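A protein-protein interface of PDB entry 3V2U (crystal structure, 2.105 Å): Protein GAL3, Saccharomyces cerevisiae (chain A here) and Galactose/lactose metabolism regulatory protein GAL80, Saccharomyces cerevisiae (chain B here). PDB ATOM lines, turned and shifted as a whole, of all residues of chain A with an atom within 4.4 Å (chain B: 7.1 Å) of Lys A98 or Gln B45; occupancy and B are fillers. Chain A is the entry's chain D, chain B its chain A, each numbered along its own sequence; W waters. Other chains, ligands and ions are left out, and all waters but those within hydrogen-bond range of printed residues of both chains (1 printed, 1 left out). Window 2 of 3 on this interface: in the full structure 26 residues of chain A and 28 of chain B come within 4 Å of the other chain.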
ATOM      1  N   SER A  84     -29.203   6.499   8.915  1.00  0.00           N
ATOM      2  CA  SER A  84     -29.183   5.703   7.709  1.00  0.00           C
ATOM      3  C   SER A  84     -30.557   5.783   7.082  1.00  0.00           C
ATOM      4  O   SER A  84     -31.530   6.133   7.747  1.00  0.00           O
ATOM      5  CB  SER A  84     -28.824   4.248   8.029  1.00  0.00           C
ATOM      6  OG  SER A  84     -29.837   3.628   8.803  1.00  0.00           O
ATOM      7  N   ILE A  85     -30.633   5.483   5.794  1.00  0.00           N
ATOM      8  CA  ILE A  85     -31.910   5.410   5.117  1.00  0.00           C
ATOM      9  C   ILE A  85     -32.097   4.045   4.489  1.00  0.00           C
ATOM     10  O   ILE A  85     -31.261   3.586   3.712  1.00  0.00           O
ATOM     11  CB  ILE A  85     -32.049   6.504   4.047  1.00  0.00           C
ATOM     12  CG1 ILE A  85     -31.968   7.876   4.714  1.00  0.00           C
ATOM     13  CG2 ILE A  85     -33.364   6.362   3.306  1.00  0.00           C
ATOM     14  CD1 ILE A  85     -32.162   9.009   3.784  1.00  0.00           C
ATOM     15  N   THR A  86     -33.194   3.395   4.854  1.00  0.00           N
ATOM     16  CA  THR A  86     -33.566   2.120   4.272  1.00  0.00           C
ATOM     17  C   THR A  86     -34.743   2.318   3.337  1.00  0.00           C
ATOM     18  O   THR A  86     -35.753   2.911   3.719  1.00  0.00           O
ATOM     19  CB  THR A  86     -33.976   1.121   5.356  1.00  0.00           C
ATOM     20  OG1 THR A  86     -32.980   1.106   6.385  1.00  0.00           O
ATOM     21  CG2 THR A  86     -34.133  -0.260   4.760  1.00  0.00           C
ATOM     22  N   ARG A  97     -32.655  -1.087  -0.621  1.00  0.00           N
ATOM     23  CA  ARG A  97     -31.378  -0.423  -0.465  1.00  0.00           C
ATOM     24  C   ARG A  97     -31.234   0.116   0.949  1.00  0.00           C
ATOM     25  O   ARG A  97     -32.225   0.339   1.649  1.00  0.00           O
ATOM     26  CB  ARG A  97     -31.207   0.717  -1.483  1.00  0.00           C
ATOM     27  CG  ARG A  97     -31.454   0.319  -2.934  1.00  0.00           C
ATOM     28  CD  ARG A  97     -30.420  -0.667  -3.461  1.00  0.00           C
ATOM     29  NE  ARG A  97     -30.676  -1.003  -4.866  1.00  0.00           N
ATOM     30  CZ  ARG A  97     -30.468  -2.201  -5.410  1.00  0.00           C
ATOM     31  NH1 ARG A  97     -30.000  -3.204  -4.676  1.00  0.00           N
ATOM     32  NH2 ARG A  97     -30.729  -2.398  -6.693  1.00  0.00           N
ATOM     33  N   LYS A  98     -29.991   0.317   1.367  1.00  0.00           N
ATOM     34  CA  LYS A  98     -29.715   0.968   2.635  1.00  0.00           C
ATOM     35  C   LYS A  98     -28.387   1.700   2.565  1.00  0.00           C
ATOM     36  O   LYS A  98     -27.361   1.120   2.189  1.00  0.00           O
ATOM     37  CB  LYS A  98     -29.691  -0.043   3.785  1.00  0.00           C
ATOM     38  CG  LYS A  98     -29.511   0.593   5.164  1.00  0.00           C
ATOM     39  CD  LYS A  98     -29.548  -0.476   6.264  1.00  0.00           C
ATOM     40  CE  LYS A  98     -29.605   0.122   7.668  1.00  0.00           C
ATOM     41  NZ  LYS A  98     -28.269   0.554   8.163  1.00  0.00           N
ATOM     42  N   PHE A  99     -28.410   2.973   2.926  1.00  0.00           N
ATOM     43  CA  PHE A  99     -27.196   3.768   2.919  1.00  0.00           C
ATOM     44  C   PHE A  99     -27.127   4.675   4.135  1.00  0.00           C
ATOM     45  O   PHE A  99     -28.120   5.280   4.524  1.00  0.00           O
ATOM     46  CB  PHE A  99     -27.073   4.577   1.619  1.00  0.00           C
ATOM     47  CG  PHE A  99     -28.358   5.192   1.161  1.00  0.00           C
ATOM     48  CD1 PHE A  99     -28.739   6.449   1.603  1.00  0.00           C
ATOM     49  CD2 PHE A  99     -29.181   4.517   0.273  1.00  0.00           C
ATOM     50  CE1 PHE A  99     -29.934   7.023   1.171  1.00  0.00           C
ATOM     51  CE2 PHE A  99     -30.369   5.078  -0.163  1.00  0.00           C
ATOM     52  CZ  PHE A  99     -30.751   6.332   0.289  1.00  0.00           C
ATOM     53  N   ASP A 100     -25.948   4.736   4.742  1.00  0.00           N
ATOM     54  CA  ASP A 100     -25.704   5.603   5.889  1.00  0.00           C
ATOM     55  C   ASP A 100     -25.427   7.033   5.428  1.00  0.00           C
ATOM     56  O   ASP A 100     -24.691   7.252   4.466  1.00  0.00           O
ATOM     57  CB  ASP A 100     -24.507   5.092   6.690  1.00  0.00           C
ATOM     58  CG  ASP A 100     -24.835   3.872   7.533  1.00  0.00           C
ATOM     59  OD1 ASP A 100     -25.931   3.300   7.367  1.00  0.00           O
ATOM     60  OD2 ASP A 100     -23.986   3.485   8.362  1.00  0.00           O
ATOM     61  N   ALA A 109     -22.793  10.878  -2.841  1.00  0.00           N
ATOM     62  CA  ALA A 109     -22.531  10.713  -4.266  1.00  0.00           C
ATOM     63  C   ALA A 109     -23.693   9.989  -4.927  1.00  0.00           C
ATOM     64  O   ALA A 109     -24.407   9.211  -4.280  1.00  0.00           O
ATOM     65  CB  ALA A 109     -21.215   9.941  -4.497  1.00  0.00           C
ATOM     66  N   LYS A 122     -32.645   9.220  -4.259  1.00  0.00           N
ATOM     67  CA  LYS A 122     -31.411   9.919  -3.913  1.00  0.00           C
ATOM     68  C   LYS A 122     -31.351  11.332  -4.481  1.00  0.00           C
ATOM     69  O   LYS A 122     -30.835  12.234  -3.830  1.00  0.00           O
ATOM     70  CB  LYS A 122     -30.173   9.105  -4.316  1.00  0.00           C
ATOM     71  CG  LYS A 122     -29.877   7.926  -3.355  1.00  0.00           C
ATOM     72  CD  LYS A 122     -28.777   7.004  -3.873  1.00  0.00           C
ATOM     73  CE  LYS A 122     -27.409   7.672  -3.868  1.00  0.00           C
ATOM     74  NZ  LYS A 122     -26.317   6.726  -4.266  1.00  0.00           N
ATOM     75  N   THR B  38     -12.061   6.730   0.490  1.00  0.00           N
ATOM     76  CA  THR B  38     -12.556   5.871  -0.579  1.00  0.00           C
ATOM     77  C   THR B  38     -13.314   4.641  -0.079  1.00  0.00           C
ATOM     78  O   THR B  38     -14.514   4.505  -0.307  1.00  0.00           O
ATOM     79  CB  THR B  38     -11.398   5.445  -1.516  1.00  0.00           C
ATOM     80  OG1 THR B  38     -10.416   4.717  -0.766  1.00  0.00           O
ATOM     81  CG2 THR B  38     -10.725   6.685  -2.137  1.00  0.00           C
ATOM     82  N   HIS B  39     -12.619   3.727   0.583  1.00  0.00           N
ATOM     83  CA  HIS B  39     -13.297   2.559   1.138  1.00  0.00           C
ATOM     84  C   HIS B  39     -14.434   2.933   2.068  1.00  0.00           C
ATOM     85  O   HIS B  39     -15.536   2.382   1.971  1.00  0.00           O
ATOM     86  CB  HIS B  39     -12.317   1.661   1.881  1.00  0.00           C
ATOM     87  CG  HIS B  39     -11.311   1.029   0.982  1.00  0.00           C
ATOM     88  ND1 HIS B  39     -11.310  -0.316   0.703  1.00  0.00           N
ATOM     89  CD2 HIS B  39     -10.301   1.567   0.263  1.00  0.00           C
ATOM     90  CE1 HIS B  39     -10.327  -0.586  -0.138  1.00  0.00           C
ATOM     91  NE2 HIS B  39      -9.698   0.538  -0.420  1.00  0.00           N
ATOM     92  N   TYR B  40     -14.169   3.865   2.972  1.00  0.00           N
ATOM     93  CA  TYR B  40     -15.164   4.202   3.982  1.00  0.00           C
ATOM     94  C   TYR B  40     -16.459   4.748   3.365  1.00  0.00           C
ATOM     95  O   TYR B  40     -17.529   4.214   3.642  1.00  0.00           O
ATOM     96  CB  TYR B  40     -14.578   5.138   5.053  1.00  0.00           C
ATOM     97  CG  TYR B  40     -15.604   5.732   5.985  1.00  0.00           C
ATOM     98  CD1 TYR B  40     -15.808   7.105   6.033  1.00  0.00           C
ATOM     99  CD2 TYR B  40     -16.372   4.919   6.816  1.00  0.00           C
ATOM    100  CE1 TYR B  40     -16.741   7.657   6.888  1.00  0.00           C
ATOM    101  CE2 TYR B  40     -17.320   5.454   7.665  1.00  0.00           C
ATOM    102  CZ  TYR B  40     -17.494   6.828   7.700  1.00  0.00           C
ATOM    103  OH  TYR B  40     -18.431   7.367   8.544  1.00  0.00           O
ATOM    104  N   PRO B  41     -16.368   5.796   2.513  1.00  0.00           N
ATOM    105  CA  PRO B  41     -17.591   6.305   1.864  1.00  0.00           C
ATOM    106  C   PRO B  41     -18.301   5.250   1.002  1.00  0.00           C
ATOM    107  O   PRO B  41     -19.529   5.271   0.877  1.00  0.00           O
ATOM    108  CB  PRO B  41     -17.081   7.464   0.990  1.00  0.00           C
ATOM    109  CG  PRO B  41     -15.801   7.888   1.621  1.00  0.00           C
ATOM    110  CD  PRO B  41     -15.191   6.635   2.225  1.00  0.00           C
ATOM    111  N   ALA B  42     -17.539   4.332   0.415  1.00  0.00           N
ATOM    112  CA  ALA B  42     -18.122   3.261  -0.397  1.00  0.00           C
ATOM    113  C   ALA B  42     -18.981   2.350   0.466  1.00  0.00           C
ATOM    114  O   ALA B  42     -20.063   1.925   0.064  1.00  0.00           O
ATOM    115  CB  ALA B  42     -17.022   2.452  -1.068  1.00  0.00           C
ATOM    116  N   ILE B  43     -18.486   2.060   1.662  1.00  0.00           N
ATOM    117  CA  ILE B  43     -19.184   1.179   2.594  1.00  0.00           C
ATOM    118  C   ILE B  43     -20.470   1.799   3.133  1.00  0.00           C
ATOM    119  O   ILE B  43     -21.490   1.121   3.258  1.00  0.00           O
ATOM    120  CB  ILE B  43     -18.238   0.744   3.728  1.00  0.00           C
ATOM    121  CG1 ILE B  43     -17.255  -0.296   3.185  1.00  0.00           C
ATOM    122  CG2 ILE B  43     -19.022   0.203   4.916  1.00  0.00           C
ATOM    123  CD1 ILE B  43     -16.137  -0.679   4.153  1.00  0.00           C
ATOM    124  N   LEU B  44     -20.437   3.097   3.414  1.00  0.00           N
ATOM    125  CA  LEU B  44     -21.635   3.796   3.873  1.00  0.00           C
ATOM    126  C   LEU B  44     -22.793   3.629   2.896  1.00  0.00           C
ATOM    127  O   LEU B  44     -23.951   3.529   3.305  1.00  0.00           O
ATOM    128  CB  LEU B  44     -21.355   5.285   4.064  1.00  0.00           C
ATOM    129  CG  LEU B  44     -20.325   5.700   5.112  1.00  0.00           C
ATOM    130  CD1 LEU B  44     -20.198   7.209   5.130  1.00  0.00           C
ATOM    131  CD2 LEU B  44     -20.707   5.172   6.496  1.00  0.00           C
ATOM    132  N   GLN B  45     -22.477   3.614   1.603  1.00  0.00           N
ATOM    133  CA  GLN B  45     -23.494   3.493   0.559  1.00  0.00           C
ATOM    134  C   GLN B  45     -24.070   2.076   0.434  1.00  0.00           C
ATOM    135  O   GLN B  45     -25.054   1.863  -0.269  1.00  0.00           O
ATOM    136  CB  GLN B  45     -22.915   3.913  -0.791  1.00  0.00           C
ATOM    137  CG  GLN B  45     -22.339   5.333  -0.810  1.00  0.00           C
ATOM    138  CD  GLN B  45     -21.861   5.753  -2.191  1.00  0.00           C
ATOM    139  OE1 GLN B  45     -22.657   5.867  -3.127  1.00  0.00           O
ATOM    140  NE2 GLN B  45     -20.553   5.982  -2.326  1.00  0.00           N
ATOM    141  N   LEU B  46     -23.447   1.114   1.107  1.00  0.00           N
ATOM    142  CA  LEU B  46     -23.789  -0.300   0.961  1.00  0.00           C
ATOM    143  C   LEU B  46     -23.920  -0.909   2.357  1.00  0.00           C
ATOM    144  O   LEU B  46     -23.420  -1.999   2.633  1.00  0.00           O
ATOM    145  CB  LEU B  46     -22.683  -1.011   0.173  1.00  0.00           C
ATOM    146  CG  LEU B  46     -22.405  -0.541  -1.267  1.00  0.00           C
ATOM    147  CD1 LEU B  46     -21.054  -1.020  -1.763  1.00  0.00           C
ATOM    148  CD2 LEU B  46     -23.492  -0.990  -2.234  1.00  0.00           C
ATOM    149  N   SER B  47     -24.583  -0.184   3.249  1.00  0.00           N
ATOM    150  CA  SER B  47     -24.481  -0.486   4.670  1.00  0.00           C
ATOM    151  C   SER B  47     -25.240  -1.736   5.088  1.00  0.00           C
ATOM    152  O   SER B  47     -25.019  -2.249   6.180  1.00  0.00           O
ATOM    153  CB  SER B  47     -24.872   0.723   5.526  1.00  0.00           C
ATOM    154  OG  SER B  47     -26.138   1.229   5.167  1.00  0.00           O
ATOM    155  N   SER B  48     -26.106  -2.245   4.218  1.00  0.00           N
ATOM    156  CA  SER B  48     -26.725  -3.539   4.475  1.00  0.00           C
ATOM    157  C   SER B  48     -25.889  -4.676   3.890  1.00  0.00           C
ATOM    158  O   SER B  48     -26.134  -5.845   4.185  1.00  0.00           O
ATOM    159  CB  SER B  48     -28.158  -3.591   3.941  1.00  0.00           C
ATOM    160  OG  SER B  48     -28.176  -3.458   2.530  1.00  0.00           O
ATOM    161  N   GLN B  49     -24.895  -4.335   3.071  1.00  0.00           N
ATOM    162  CA  GLN B  49     -24.058  -5.364   2.459  1.00  0.00           C
ATOM    163  C   GLN B  49     -22.713  -5.543   3.150  1.00  0.00           C
ATOM    164  O   GLN B  49     -22.145  -6.632   3.134  1.00  0.00           O
ATOM    165  CB  GLN B  49     -23.859  -5.085   0.972  1.00  0.00           C
ATOM    166  CG  GLN B  49     -25.104  -5.327   0.147  1.00  0.00           C
ATOM    167  CD  GLN B  49     -25.383  -4.183  -0.787  1.00  0.00           C
ATOM    168  OE1 GLN B  49     -25.918  -3.154  -0.374  1.00  0.00           O
ATOM    169  NE2 GLN B  49     -25.007  -4.342  -2.054  1.00  0.00           N
ATOM    170  N   GLN B  51     -20.448  -4.306   6.793  1.00  0.00           N
ATOM    171  CA  GLN B  51     -20.398  -3.632   8.078  1.00  0.00           C
ATOM    172  C   GLN B  51     -18.978  -3.708   8.587  1.00  0.00           C
ATOM    173  O   GLN B  51     -18.326  -4.739   8.443  1.00  0.00           O
ATOM    174  CB  GLN B  51     -21.349  -4.303   9.089  1.00  0.00           C
ATOM    175  CG  GLN B  51     -22.778  -3.804   8.988  1.00  0.00           C
ATOM    176  CD  GLN B  51     -22.883  -2.308   9.237  1.00  0.00           C
ATOM    177  OE1 GLN B  51     -23.428  -1.550   8.420  1.00  0.00           O
ATOM    178  NE2 GLN B  51     -22.359  -1.874  10.373  1.00  0.00           N
ATOM    179  N   VAL B 365     -14.532   8.319  -5.110  1.00  0.00           N
ATOM    180  CA  VAL B 365     -15.410   7.442  -4.347  1.00  0.00           C
ATOM    181  C   VAL B 365     -16.059   6.393  -5.265  1.00  0.00           C
ATOM    182  O   VAL B 365     -16.141   5.209  -4.923  1.00  0.00           O
ATOM    183  CB  VAL B 365     -16.478   8.271  -3.627  1.00  0.00           C
ATOM    184  CG1 VAL B 365     -17.536   7.372  -2.968  1.00  0.00           C
ATOM    185  CG2 VAL B 365     -15.824   9.186  -2.609  1.00  0.00           C
ATOM    186  N   GLY B 366     -16.468   6.827  -6.453  1.00  0.00           N
ATOM    187  CA  GLY B 366     -17.263   5.991  -7.336  1.00  0.00           C
ATOM    188  C   GLY B 366     -16.599   4.719  -7.849  1.00  0.00           C
ATOM    189  O   GLY B 366     -17.235   3.668  -7.942  1.00  0.00           O
ATOM    190  N   HIS B 369     -16.378   2.306  -5.010  1.00  0.00           N
ATOM    191  CA  HIS B 369     -17.725   1.921  -4.696  1.00  0.00           C
ATOM    192  C   HIS B 369     -18.225   0.813  -5.621  1.00  0.00           C
ATOM    193  O   HIS B 369     -18.889  -0.123  -5.175  1.00  0.00           O
ATOM    194  CB  HIS B 369     -18.658   3.123  -4.790  1.00  0.00           C
ATOM    195  CG  HIS B 369     -20.103   2.753  -4.710  1.00  0.00           C
ATOM    196  ND1 HIS B 369     -20.923   2.719  -5.817  1.00  0.00           N
ATOM    197  CD2 HIS B 369     -20.865   2.365  -3.662  1.00  0.00           C
ATOM    198  CE1 HIS B 369     -22.136   2.354  -5.447  1.00  0.00           C
ATOM    199  NE2 HIS B 369     -22.130   2.128  -4.148  1.00  0.00           N
ATOM    200  N   GLN B 373     -19.370  -2.991  -4.825  1.00  0.00           N
ATOM    201  CA  GLN B 373     -20.622  -3.462  -5.383  1.00  0.00           C
ATOM    202  C   GLN B 373     -20.410  -4.835  -6.043  1.00  0.00           C
ATOM    203  O   GLN B 373     -21.236  -5.741  -5.887  1.00  0.00           O
ATOM    204  CB  GLN B 373     -21.090  -2.457  -6.426  1.00  0.00           C
ATOM    205  CG  GLN B 373     -22.567  -2.215  -6.518  1.00  0.00           C
ATOM    206  CD  GLN B 373     -22.891  -0.825  -7.054  1.00  0.00           C
ATOM    207  OE1 GLN B 373     -22.048  -0.145  -7.660  1.00  0.00           O
ATOM    208  NE2 GLN B 373     -24.114  -0.389  -6.819  1.00  0.00           N
HETATM  209  O   HOH W   1     -27.669   0.521  -0.764  1.00  0.00           O
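Of the printed residues of chain B, Lys A98 touches Gln B45 (3.5 Å), Leu B46 (3.998 Å), Ser B47 (3.2 Å) and Ser B48 (3.9 Å).
Printed residues of chain B within 4 Å of Asp A100: Leu B44 (2.7 Å) and Ser B47 (3.0 Å).
Of the printed residues of chain B, Ala A109 touches Gln B45 (3.9 Å).
Printed residues of chain B within 4 Å of Lys A122: Gln B45 (3.9 Å).
Pro B41 touches none of the printed residues of chain A.
Of the printed residues of chain A, Leu B44 touches Phe A99 and Asp A100.
The nearest printed residue of chain B that does not touch Lys A98 is Leu B44 (4.3 Å).
The nearest printed residue of chain B that does not touch Ala A109 is Val B365 (4.7 Å).
Of the 9 printed residues of chain A, 5 touch a printed residue of chain B.
Of the 17 printed residues of chain B, 5 touch a printed residue of chain A.
Hydrophobic or aromatic side chains of chain B that line the printed part of chain A: Leu B44.
Water W1 bridges the backbone carbonyl oxygen (O) of Gln B45 (3.0 Å) and the backbone carbonyl oxygen (O) of Lys A98 (3.0 Å).
Among the printed residues, merely in contact across the chains: Phe A99 with Leu B44 (3.3 Å), Phe A99 with Ser B47 (3.6 Å), Lys A98 with Ser B48 (3.9 Å), Phe A99 with Gln B45 (3.9 Å), Lys A122 with Gln B45 (3.9 Å), Ala A109 with Gln B45 (3.9 Å) and Lys A98 with Leu B46 (3.998 Å).
N of Asp A100 lies within hydrogen-bond range of O of Leu B44, at 2.7 Å.
OG of Ser B47 is in hydrogen-bond range of O of Lys A98 (3.2 Å).
The side-chain carboxylate of Asp A100 sits at hydrogen-bond distance from the side-chain hydroxyl of Ser B47 (3.0 Å).
O of Lys A98 sits close to O of Gln B45 (3.5 Å).
The backbone carbonyl oxygen of Pro B41 lies close to the side-chain amide nitrogen of Gln B45 (3.4 Å).
The backbone carbonyl oxygen (O) of Ser B47 sits close to the side-chain amide oxygen (OE1) of Gln B51 (2.8 Å).
N of Ile A85 lies within hydrogen-bond range of O of Phe A99, 2.8 Å away.
The side-chain carboxylate of Asp A100 is in salt-bridge range of the side-chain amino group of Lys A98.
O of Ala A109 lies within hydrogen-bond range of NZ of Lys A122 (3.1 Å).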
